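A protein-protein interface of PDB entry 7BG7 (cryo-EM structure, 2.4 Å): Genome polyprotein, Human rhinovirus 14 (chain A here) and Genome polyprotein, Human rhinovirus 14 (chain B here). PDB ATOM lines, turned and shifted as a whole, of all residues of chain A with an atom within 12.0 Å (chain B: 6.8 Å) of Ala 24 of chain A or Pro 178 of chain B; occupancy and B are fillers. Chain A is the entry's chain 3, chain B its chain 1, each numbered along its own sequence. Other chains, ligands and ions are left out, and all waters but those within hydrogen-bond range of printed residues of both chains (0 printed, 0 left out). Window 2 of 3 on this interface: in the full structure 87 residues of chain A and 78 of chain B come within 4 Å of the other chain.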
ATOM      1  N   GLN A  20      -6.899 -19.782  -7.334  1.00  0.00           N
ATOM      2  CA  GLN A  20      -8.042 -19.217  -8.036  1.00  0.00           C
ATOM      3  C   GLN A  20      -7.566 -18.508  -9.295  1.00  0.00           C
ATOM      4  O   GLN A  20      -6.435 -18.028  -9.369  1.00  0.00           O
ATOM      5  CB  GLN A  20      -8.790 -18.230  -7.142  1.00  0.00           C
ATOM      6  CG  GLN A  20      -9.328 -18.814  -5.853  1.00  0.00           C
ATOM      7  CD  GLN A  20      -9.942 -17.758  -4.950  1.00  0.00           C
ATOM      8  OE1 GLN A  20     -10.820 -17.006  -5.359  1.00  0.00           O
ATOM      9  NE2 GLN A  20      -9.471 -17.696  -3.712  1.00  0.00           N
ATOM     10  N   SER A  21      -8.438 -18.451 -10.296  1.00  0.00           N
ATOM     11  CA  SER A  21      -8.107 -17.784 -11.547  1.00  0.00           C
ATOM     12  C   SER A  21      -9.362 -17.180 -12.149  1.00  0.00           C
ATOM     13  O   SER A  21     -10.462 -17.700 -11.934  1.00  0.00           O
ATOM     14  CB  SER A  21      -7.451 -18.745 -12.552  1.00  0.00           C
ATOM     15  OG  SER A  21      -8.345 -19.752 -12.978  1.00  0.00           O
ATOM     16  N   PRO A  22      -9.238 -16.087 -12.892  1.00  0.00           N
ATOM     17  CA  PRO A  22     -10.426 -15.464 -13.477  1.00  0.00           C
ATOM     18  C   PRO A  22     -11.066 -16.355 -14.528  1.00  0.00           C
ATOM     19  O   PRO A  22     -10.395 -17.087 -15.258  1.00  0.00           O
ATOM     20  CB  PRO A  22      -9.881 -14.174 -14.098  1.00  0.00           C
ATOM     21  CG  PRO A  22      -8.449 -14.465 -14.347  1.00  0.00           C
ATOM     22  CD  PRO A  22      -8.008 -15.368 -13.255  1.00  0.00           C
ATOM     23  N   SER A  23     -12.385 -16.273 -14.604  1.00  0.00           N
ATOM     24  CA  SER A  23     -13.149 -17.061 -15.554  1.00  0.00           C
ATOM     25  C   SER A  23     -13.249 -16.338 -16.892  1.00  0.00           C
ATOM     26  O   SER A  23     -13.469 -15.128 -16.943  1.00  0.00           O
ATOM     27  CB  SER A  23     -14.546 -17.330 -14.995  1.00  0.00           C
ATOM     28  OG  SER A  23     -15.272 -18.223 -15.814  1.00  0.00           O
ATOM     29  N   ALA A  24     -13.093 -17.095 -17.973  1.00  0.00           N
ATOM     30  CA  ALA A  24     -13.218 -16.540 -19.313  1.00  0.00           C
ATOM     31  C   ALA A  24     -14.670 -16.458 -19.754  1.00  0.00           C
ATOM     32  O   ALA A  24     -14.982 -15.727 -20.696  1.00  0.00           O
ATOM     33  CB  ALA A  24     -12.419 -17.378 -20.309  1.00  0.00           C
ATOM     34  N   LEU A  25     -15.559 -17.199 -19.096  1.00  0.00           N
ATOM     35  CA  LEU A  25     -16.984 -17.205 -19.400  1.00  0.00           C
ATOM     36  C   LEU A  25     -17.744 -16.777 -18.153  1.00  0.00           C
ATOM     37  O   LEU A  25     -18.377 -17.603 -17.482  1.00  0.00           O
ATOM     38  CB  LEU A  25     -17.440 -18.591 -19.849  1.00  0.00           C
ATOM     39  CG  LEU A  25     -16.737 -19.171 -21.071  1.00  0.00           C
ATOM     40  CD1 LEU A  25     -17.309 -20.536 -21.410  1.00  0.00           C
ATOM     41  CD2 LEU A  25     -16.854 -18.228 -22.245  1.00  0.00           C
ATOM     42  N   PRO A  26     -17.709 -15.490 -17.820  1.00  0.00           N
ATOM     43  CA  PRO A  26     -18.443 -15.027 -16.641  1.00  0.00           C
ATOM     44  C   PRO A  26     -19.935 -15.226 -16.830  1.00  0.00           C
ATOM     45  O   PRO A  26     -20.467 -15.067 -17.929  1.00  0.00           O
ATOM     46  CB  PRO A  26     -18.069 -13.543 -16.548  1.00  0.00           C
ATOM     47  CG  PRO A  26     -17.640 -13.173 -17.910  1.00  0.00           C
ATOM     48  CD  PRO A  26     -17.013 -14.388 -18.500  1.00  0.00           C
ATOM     49  N   ASN A  27     -20.598 -15.636 -15.753  1.00  0.00           N
ATOM     50  CA  ASN A  27     -22.042 -15.772 -15.663  1.00  0.00           C
ATOM     51  C   ASN A  27     -22.538 -17.011 -16.393  1.00  0.00           C
ATOM     52  O   ASN A  27     -23.752 -17.188 -16.524  1.00  0.00           O
ATOM     53  CB  ASN A  27     -22.767 -14.535 -16.194  1.00  0.00           C
ATOM     54  CG  ASN A  27     -22.455 -13.307 -15.384  1.00  0.00           C
ATOM     55  OD1 ASN A  27     -22.840 -13.204 -14.223  1.00  0.00           O
ATOM     56  ND2 ASN A  27     -21.754 -12.362 -15.989  1.00  0.00           N
ATOM     57  N   TYR A  28     -21.641 -17.860 -16.880  1.00  0.00           N
ATOM     58  CA  TYR A  28     -22.037 -19.086 -17.554  1.00  0.00           C
ATOM     59  C   TYR A  28     -22.625 -20.060 -16.544  1.00  0.00           C
ATOM     60  O   TYR A  28     -22.094 -20.227 -15.446  1.00  0.00           O
ATOM     61  CB  TYR A  28     -20.847 -19.721 -18.271  1.00  0.00           C
ATOM     62  CG  TYR A  28     -21.176 -21.044 -18.915  1.00  0.00           C
ATOM     63  CD1 TYR A  28     -21.622 -21.110 -20.225  1.00  0.00           C
ATOM     64  CD2 TYR A  28     -21.056 -22.227 -18.203  1.00  0.00           C
ATOM     65  CE1 TYR A  28     -21.933 -22.316 -20.806  1.00  0.00           C
ATOM     66  CE2 TYR A  28     -21.357 -23.435 -18.778  1.00  0.00           C
ATOM     67  CZ  TYR A  28     -21.795 -23.474 -20.079  1.00  0.00           C
ATOM     68  OH  TYR A  28     -22.102 -24.679 -20.650  1.00  0.00           O
ATOM     69  N   GLU A  29     -23.741 -20.674 -16.906  1.00  0.00           N
ATOM     70  CA  GLU A  29     -24.417 -21.643 -16.053  1.00  0.00           C
ATOM     71  C   GLU A  29     -24.271 -23.036 -16.648  1.00  0.00           C
ATOM     72  O   GLU A  29     -24.886 -23.332 -17.684  1.00  0.00           O
ATOM     73  CB  GLU A  29     -25.889 -21.268 -15.892  1.00  0.00           C
ATOM     74  CG  GLU A  29     -26.070 -19.931 -15.190  1.00  0.00           C
ATOM     75  CD  GLU A  29     -27.517 -19.558 -14.961  1.00  0.00           C
ATOM     76  OE1 GLU A  29     -28.168 -19.065 -15.898  1.00  0.00           O
ATOM     77  OE2 GLU A  29     -28.015 -19.788 -13.842  1.00  0.00           O
ATOM     78  N   PRO A  30     -23.447 -23.903 -16.065  1.00  0.00           N
ATOM     79  CA  PRO A  30     -23.254 -25.242 -16.633  1.00  0.00           C
ATOM     80  C   PRO A  30     -24.470 -26.137 -16.460  1.00  0.00           C
ATOM     81  O   PRO A  30     -25.306 -25.942 -15.579  1.00  0.00           O
ATOM     82  CB  PRO A  30     -22.054 -25.782 -15.855  1.00  0.00           C
ATOM     83  CG  PRO A  30     -22.093 -25.067 -14.573  1.00  0.00           C
ATOM     84  CD  PRO A  30     -22.642 -23.705 -14.849  1.00  0.00           C
ATOM     85  N   GLN B 153      -1.991 -12.772 -28.415  1.00  0.00           N
ATOM     86  CA  GLN B 153      -3.429 -12.808 -28.182  1.00  0.00           C
ATOM     87  C   GLN B 153      -3.874 -14.265 -28.262  1.00  0.00           C
ATOM     88  O   GLN B 153      -3.783 -14.886 -29.323  1.00  0.00           O
ATOM     89  CB  GLN B 153      -4.192 -11.952 -29.188  1.00  0.00           C
ATOM     90  CG  GLN B 153      -5.695 -12.009 -28.979  1.00  0.00           C
ATOM     91  CD  GLN B 153      -6.472 -11.119 -29.916  1.00  0.00           C
ATOM     92  OE1 GLN B 153      -5.912 -10.515 -30.824  1.00  0.00           O
ATOM     93  NE2 GLN B 153      -7.781 -11.061 -29.719  1.00  0.00           N
ATOM     94  N   ALA B 154      -4.341 -14.807 -27.147  1.00  0.00           N
ATOM     95  CA  ALA B 154      -4.963 -16.125 -27.112  1.00  0.00           C
ATOM     96  C   ALA B 154      -6.469 -15.923 -27.020  1.00  0.00           C
ATOM     97  O   ALA B 154      -6.978 -15.442 -26.003  1.00  0.00           O
ATOM     98  CB  ALA B 154      -4.445 -16.957 -25.943  1.00  0.00           C
ATOM     99  N   MET B 155      -7.177 -16.267 -28.084  1.00  0.00           N
ATOM    100  CA  MET B 155      -8.611 -16.058 -28.169  1.00  0.00           C
ATOM    101  C   MET B 155      -9.321 -17.391 -28.030  1.00  0.00           C
ATOM    102  O   MET B 155      -9.172 -18.275 -28.878  1.00  0.00           O
ATOM    103  CB  MET B 155      -8.983 -15.389 -29.489  1.00  0.00           C
ATOM    104  CG  MET B 155     -10.447 -14.976 -29.583  1.00  0.00           C
ATOM    105  SD  MET B 155     -10.762 -13.799 -30.907  1.00  0.00           S
ATOM    106  CE  MET B 155     -10.441 -14.828 -32.325  1.00  0.00           C
ATOM    107  N   TYR B 156     -10.087 -17.531 -26.963  1.00  0.00           N
ATOM    108  CA  TYR B 156     -10.995 -18.654 -26.822  1.00  0.00           C
ATOM    109  C   TYR B 156     -12.221 -18.389 -27.682  1.00  0.00           C
ATOM    110  O   TYR B 156     -12.946 -17.420 -27.447  1.00  0.00           O
ATOM    111  CB  TYR B 156     -11.389 -18.848 -25.364  1.00  0.00           C
ATOM    112  CG  TYR B 156     -12.417 -19.925 -25.157  1.00  0.00           C
ATOM    113  CD1 TYR B 156     -12.040 -21.226 -24.863  1.00  0.00           C
ATOM    114  CD2 TYR B 156     -13.766 -19.645 -25.265  1.00  0.00           C
ATOM    115  CE1 TYR B 156     -12.979 -22.208 -24.673  1.00  0.00           C
ATOM    116  CE2 TYR B 156     -14.712 -20.623 -25.082  1.00  0.00           C
ATOM    117  CZ  TYR B 156     -14.314 -21.904 -24.789  1.00  0.00           C
ATOM    118  OH  TYR B 156     -15.261 -22.878 -24.601  1.00  0.00           O
ATOM    119  N   VAL B 157     -12.432 -19.209 -28.697  1.00  0.00           N
ATOM    120  CA  VAL B 157     -13.621 -19.125 -29.541  1.00  0.00           C
ATOM    121  C   VAL B 157     -14.617 -20.176 -29.060  1.00  0.00           C
ATOM    122  O   VAL B 157     -14.230 -21.340 -28.890  1.00  0.00           O
ATOM    123  CB  VAL B 157     -13.287 -19.322 -31.031  1.00  0.00           C
ATOM    124  CG1 VAL B 157     -12.084 -18.493 -31.426  1.00  0.00           C
ATOM    125  CG2 VAL B 157     -13.048 -20.734 -31.319  1.00  0.00           C
ATOM    126  N   PRO B 158     -15.868 -19.812 -28.791  1.00  0.00           N
ATOM    127  CA  PRO B 158     -16.873 -20.803 -28.384  1.00  0.00           C
ATOM    128  C   PRO B 158     -17.046 -21.894 -29.426  1.00  0.00           C
ATOM    129  O   PRO B 158     -16.764 -21.678 -30.613  1.00  0.00           O
ATOM    130  CB  PRO B 158     -18.150 -19.963 -28.243  1.00  0.00           C
ATOM    131  CG  PRO B 158     -17.664 -18.610 -27.962  1.00  0.00           C
ATOM    132  CD  PRO B 158     -16.431 -18.452 -28.781  1.00  0.00           C
ATOM    133  N   SER B 174     -13.312  -9.501 -31.829  1.00  0.00           N
ATOM    134  CA  SER B 174     -14.632  -9.978 -31.451  1.00  0.00           C
ATOM    135  C   SER B 174     -15.077  -9.374 -30.128  1.00  0.00           C
ATOM    136  O   SER B 174     -14.351  -9.417 -29.133  1.00  0.00           O
ATOM    137  CB  SER B 174     -14.626 -11.502 -31.363  1.00  0.00           C
ATOM    138  OG  SER B 174     -15.881 -11.992 -30.932  1.00  0.00           O
ATOM    139  N   ALA B 175     -16.282  -8.823 -30.115  1.00  0.00           N
ATOM    140  CA  ALA B 175     -16.820  -8.203 -28.916  1.00  0.00           C
ATOM    141  C   ALA B 175     -17.333  -9.238 -27.925  1.00  0.00           C
ATOM    142  O   ALA B 175     -17.812  -8.858 -26.852  1.00  0.00           O
ATOM    143  CB  ALA B 175     -17.943  -7.227 -29.279  1.00  0.00           C
ATOM    144  N   SER B 176     -17.258 -10.523 -28.260  1.00  0.00           N
ATOM    145  CA  SER B 176     -17.831 -11.598 -27.458  1.00  0.00           C
ATOM    146  C   SER B 176     -16.820 -12.685 -27.122  1.00  0.00           C
ATOM    147  O   SER B 176     -16.888 -13.249 -26.032  1.00  0.00           O
ATOM    148  CB  SER B 176     -19.034 -12.230 -28.173  1.00  0.00           C
ATOM    149  OG  SER B 176     -20.170 -11.388 -28.102  1.00  0.00           O
ATOM    150  N   ASN B 177     -15.895 -12.995 -28.022  1.00  0.00           N
ATOM    151  CA  ASN B 177     -14.930 -14.060 -27.756  1.00  0.00           C
ATOM    152  C   ASN B 177     -13.991 -13.640 -26.630  1.00  0.00           C
ATOM    153  O   ASN B 177     -13.385 -12.568 -26.706  1.00  0.00           O
ATOM    154  CB  ASN B 177     -14.111 -14.387 -29.000  1.00  0.00           C
ATOM    155  CG  ASN B 177     -14.950 -14.929 -30.132  1.00  0.00           C
ATOM    156  OD1 ASN B 177     -16.030 -15.467 -29.923  1.00  0.00           O
ATOM    157  ND2 ASN B 177     -14.457 -14.773 -31.347  1.00  0.00           N
ATOM    158  N   PRO B 178     -13.846 -14.439 -25.575  1.00  0.00           N
ATOM    159  CA  PRO B 178     -12.838 -14.129 -24.553  1.00  0.00           C
ATOM    160  C   PRO B 178     -11.439 -14.140 -25.148  1.00  0.00           C
ATOM    161  O   PRO B 178     -11.066 -15.057 -25.879  1.00  0.00           O
ATOM    162  CB  PRO B 178     -13.020 -15.247 -23.521  1.00  0.00           C
ATOM    163  CG  PRO B 178     -14.375 -15.757 -23.751  1.00  0.00           C
ATOM    164  CD  PRO B 178     -14.632 -15.627 -25.209  1.00  0.00           C
ATOM    165  N   SER B 179     -10.671 -13.104 -24.843  1.00  0.00           N
ATOM    166  CA  SER B 179      -9.295 -12.994 -25.303  1.00  0.00           C
ATOM    167  C   SER B 179      -8.404 -12.557 -24.157  1.00  0.00           C
ATOM    168  O   SER B 179      -8.827 -11.801 -23.281  1.00  0.00           O
ATOM    169  CB  SER B 179      -9.155 -12.012 -26.461  1.00  0.00           C
ATOM    170  OG  SER B 179      -9.767 -12.525 -27.622  1.00  0.00           O
ATOM    171  N   VAL B 180      -7.185 -13.076 -24.146  1.00  0.00           N
ATOM    172  CA  VAL B 180      -6.178 -12.700 -23.168  1.00  0.00           C
ATOM    173  C   VAL B 180      -4.930 -12.242 -23.911  1.00  0.00           C
ATOM    174  O   VAL B 180      -4.472 -12.911 -24.841  1.00  0.00           O
ATOM    175  CB  VAL B 180      -5.871 -13.849 -22.185  1.00  0.00           C
ATOM    176  CG1 VAL B 180      -5.347 -15.081 -22.910  1.00  0.00           C
ATOM    177  CG2 VAL B 180      -4.910 -13.374 -21.107  1.00  0.00           C
ATOM    178  N   PHE B 190      -6.471 -18.483 -17.080  1.00  0.00           N
ATOM    179  CA  PHE B 190      -7.897 -18.226 -17.035  1.00  0.00           C
ATOM    180  C   PHE B 190      -8.622 -19.559 -16.937  1.00  0.00           C
ATOM    181  O   PHE B 190      -8.167 -20.561 -17.487  1.00  0.00           O
ATOM    182  CB  PHE B 190      -8.356 -17.451 -18.275  1.00  0.00           C
ATOM    183  CG  PHE B 190      -8.052 -18.142 -19.566  1.00  0.00           C
ATOM    184  CD1 PHE B 190      -8.976 -18.992 -20.147  1.00  0.00           C
ATOM    185  CD2 PHE B 190      -6.849 -17.940 -20.207  1.00  0.00           C
ATOM    186  CE1 PHE B 190      -8.700 -19.623 -21.342  1.00  0.00           C
ATOM    187  CE2 PHE B 190      -6.566 -18.572 -21.401  1.00  0.00           C
ATOM    188  CZ  PHE B 190      -7.495 -19.417 -21.967  1.00  0.00           C
ATOM    189  N   SER B 191      -9.724 -19.565 -16.211  1.00  0.00           N
ATOM    190  CA  SER B 191     -10.535 -20.756 -16.045  1.00  0.00           C
ATOM    191  C   SER B 191     -11.698 -20.708 -17.023  1.00  0.00           C
ATOM    192  O   SER B 191     -12.201 -19.638 -17.369  1.00  0.00           O
ATOM    193  CB  SER B 191     -11.064 -20.881 -14.617  1.00  0.00           C
ATOM    194  OG  SER B 191     -11.976 -19.850 -14.304  1.00  0.00           O
ATOM    195  N   VAL B 192     -12.090 -21.879 -17.512  1.00  0.00           N
ATOM    196  CA  VAL B 192     -13.289 -22.037 -18.321  1.00  0.00           C
ATOM    197  C   VAL B 192     -14.192 -23.022 -17.594  1.00  0.00           C
ATOM    198  O   VAL B 192     -13.738 -24.108 -17.233  1.00  0.00           O
ATOM    199  CB  VAL B 192     -12.988 -22.546 -19.743  1.00  0.00           C
ATOM    200  CG1 VAL B 192     -14.267 -22.645 -20.536  1.00  0.00           C
ATOM    201  CG2 VAL B 192     -12.009 -21.642 -20.444  1.00  0.00           C
ATOM    202  N   PRO B 193     -15.451 -22.686 -17.329  1.00  0.00           N
ATOM    203  CA  PRO B 193     -16.339 -23.643 -16.670  1.00  0.00           C
ATOM    204  C   PRO B 193     -16.598 -24.843 -17.568  1.00  0.00           C
ATOM    205  O   PRO B 193     -16.248 -24.867 -18.747  1.00  0.00           O
ATOM    206  CB  PRO B 193     -17.618 -22.839 -16.420  1.00  0.00           C
ATOM    207  CG  PRO B 193     -17.575 -21.738 -17.401  1.00  0.00           C
ATOM    208  CD  PRO B 193     -16.134 -21.410 -17.604  1.00  0.00           C
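The backbone NH of Ser 191 of chain B is in hydrogen-bond range of the backbone carbonyl oxygen of Pro 22 of chain A (2.7 Å). O of Ser 191 of chain B is in hydrogen-bond range of N of Ala 24 of chain A (2.8 Å).
The backbone carbonyl oxygen (O) of Pro 178 of chain B sits at hydrogen-bond distance from the backbone NH (N) of Tyr 156 of chain B (2.9 Å). N of Leu 25 of chain A sits close to OG of Ser 23 of chain A (3.4 Å).
Among the printed residues, pairs that only touch across the chains: Ser 21 of chain A with Phe 190 of chain B (3.97 Å), Ser 21 of chain A with Ser 191 of chain B (3.4 Å), Pro 22 of chain A with Phe 190 of chain B (3.3 Å), Ser 23 of chain A with Ser 191 of chain B (3.3 Å), Ser 23 of chain A with Pro 193 of chain B (3.8 Å), Ala 24 of chain A with Pro 178 of chain B (3.1 Å), Ala 24 of chain A with Phe 190 of chain B (3.8 Å), Leu 25 of chain A with Pro 178 of chain B (3.8 Å), Leu 25 of chain A with Val 192 of chain B (3.8 Å), Leu 25 of chain A with Pro 193 of chain B (3.8 Å) and Tyr 28 of chain A with Pro 193 of chain B (3.6 Å).
Of the printed residues of chain A, Pro 178 of chain B touches Ala 24 (3.1 Å) and Leu 25 (3.8 Å). No residue of chain A comes within 4 Å of Met 155 of chain B. No residue of chain A comes within 4 Å of Ser 176 of chain B. No residue of chain A comes within 4 Å of Asn 177 of chain B. Ser 179 of chain B touches none of the printed residues of chain A. Val 180 of chain B touches none of the printed residues of chain A. Phe 190 of chain B touches three residues of chain A. Of chain A, only Ser 21, Pro 22, Ser 23 and Ala 24 come within 4 Å of Ser 191 of chain B. Val 192 of chain B touches just one residue of chain A: Leu 25 (3.8 Å). Of the printed residues of chain B, Tyr 28 of chain A touches Pro 193. Printed residues of chain B within 4 Å of Ser 23 of chain A: Ser 191 (3.3 Å) and Pro 193 (3.8 Å). Printed residues of chain B within 4 Å of Leu 25 of chain A: Pro 178, Val 192 and Pro 193. Of the printed residues of chain A, Pro 193 of chain B touches Ser 23, Leu 25 and Tyr 28. Of the printed residues of chain B, Ser 21 of chain A touches Phe 190 and Ser 191. Val 157 of chain B touches none of the printed residues of chain A. The nearest residue of chain A that does not touch Pro 178 of chain B is Pro 26 of chain A (6.0 Å).
Of the 17 printed residues of chain B, 5 touch a printed residue of chain A. Hydrophobic or aromatic side chains of chain B that line the printed part of chain A: Pro 178, Phe 190, Val 192 and Pro 193. Printed residues of chain A that touch a printed residue of chain B: Ser 21, Pro 22, Ser 23, Ala 24, Leu 25 and Tyr 28. Among the printed residues, 13 pairs touch across the chains. Among the printed residues, no Asp or Glu carboxylate lies within 4 Å of a Lys or Arg side-chain nitrogen of the other chain.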
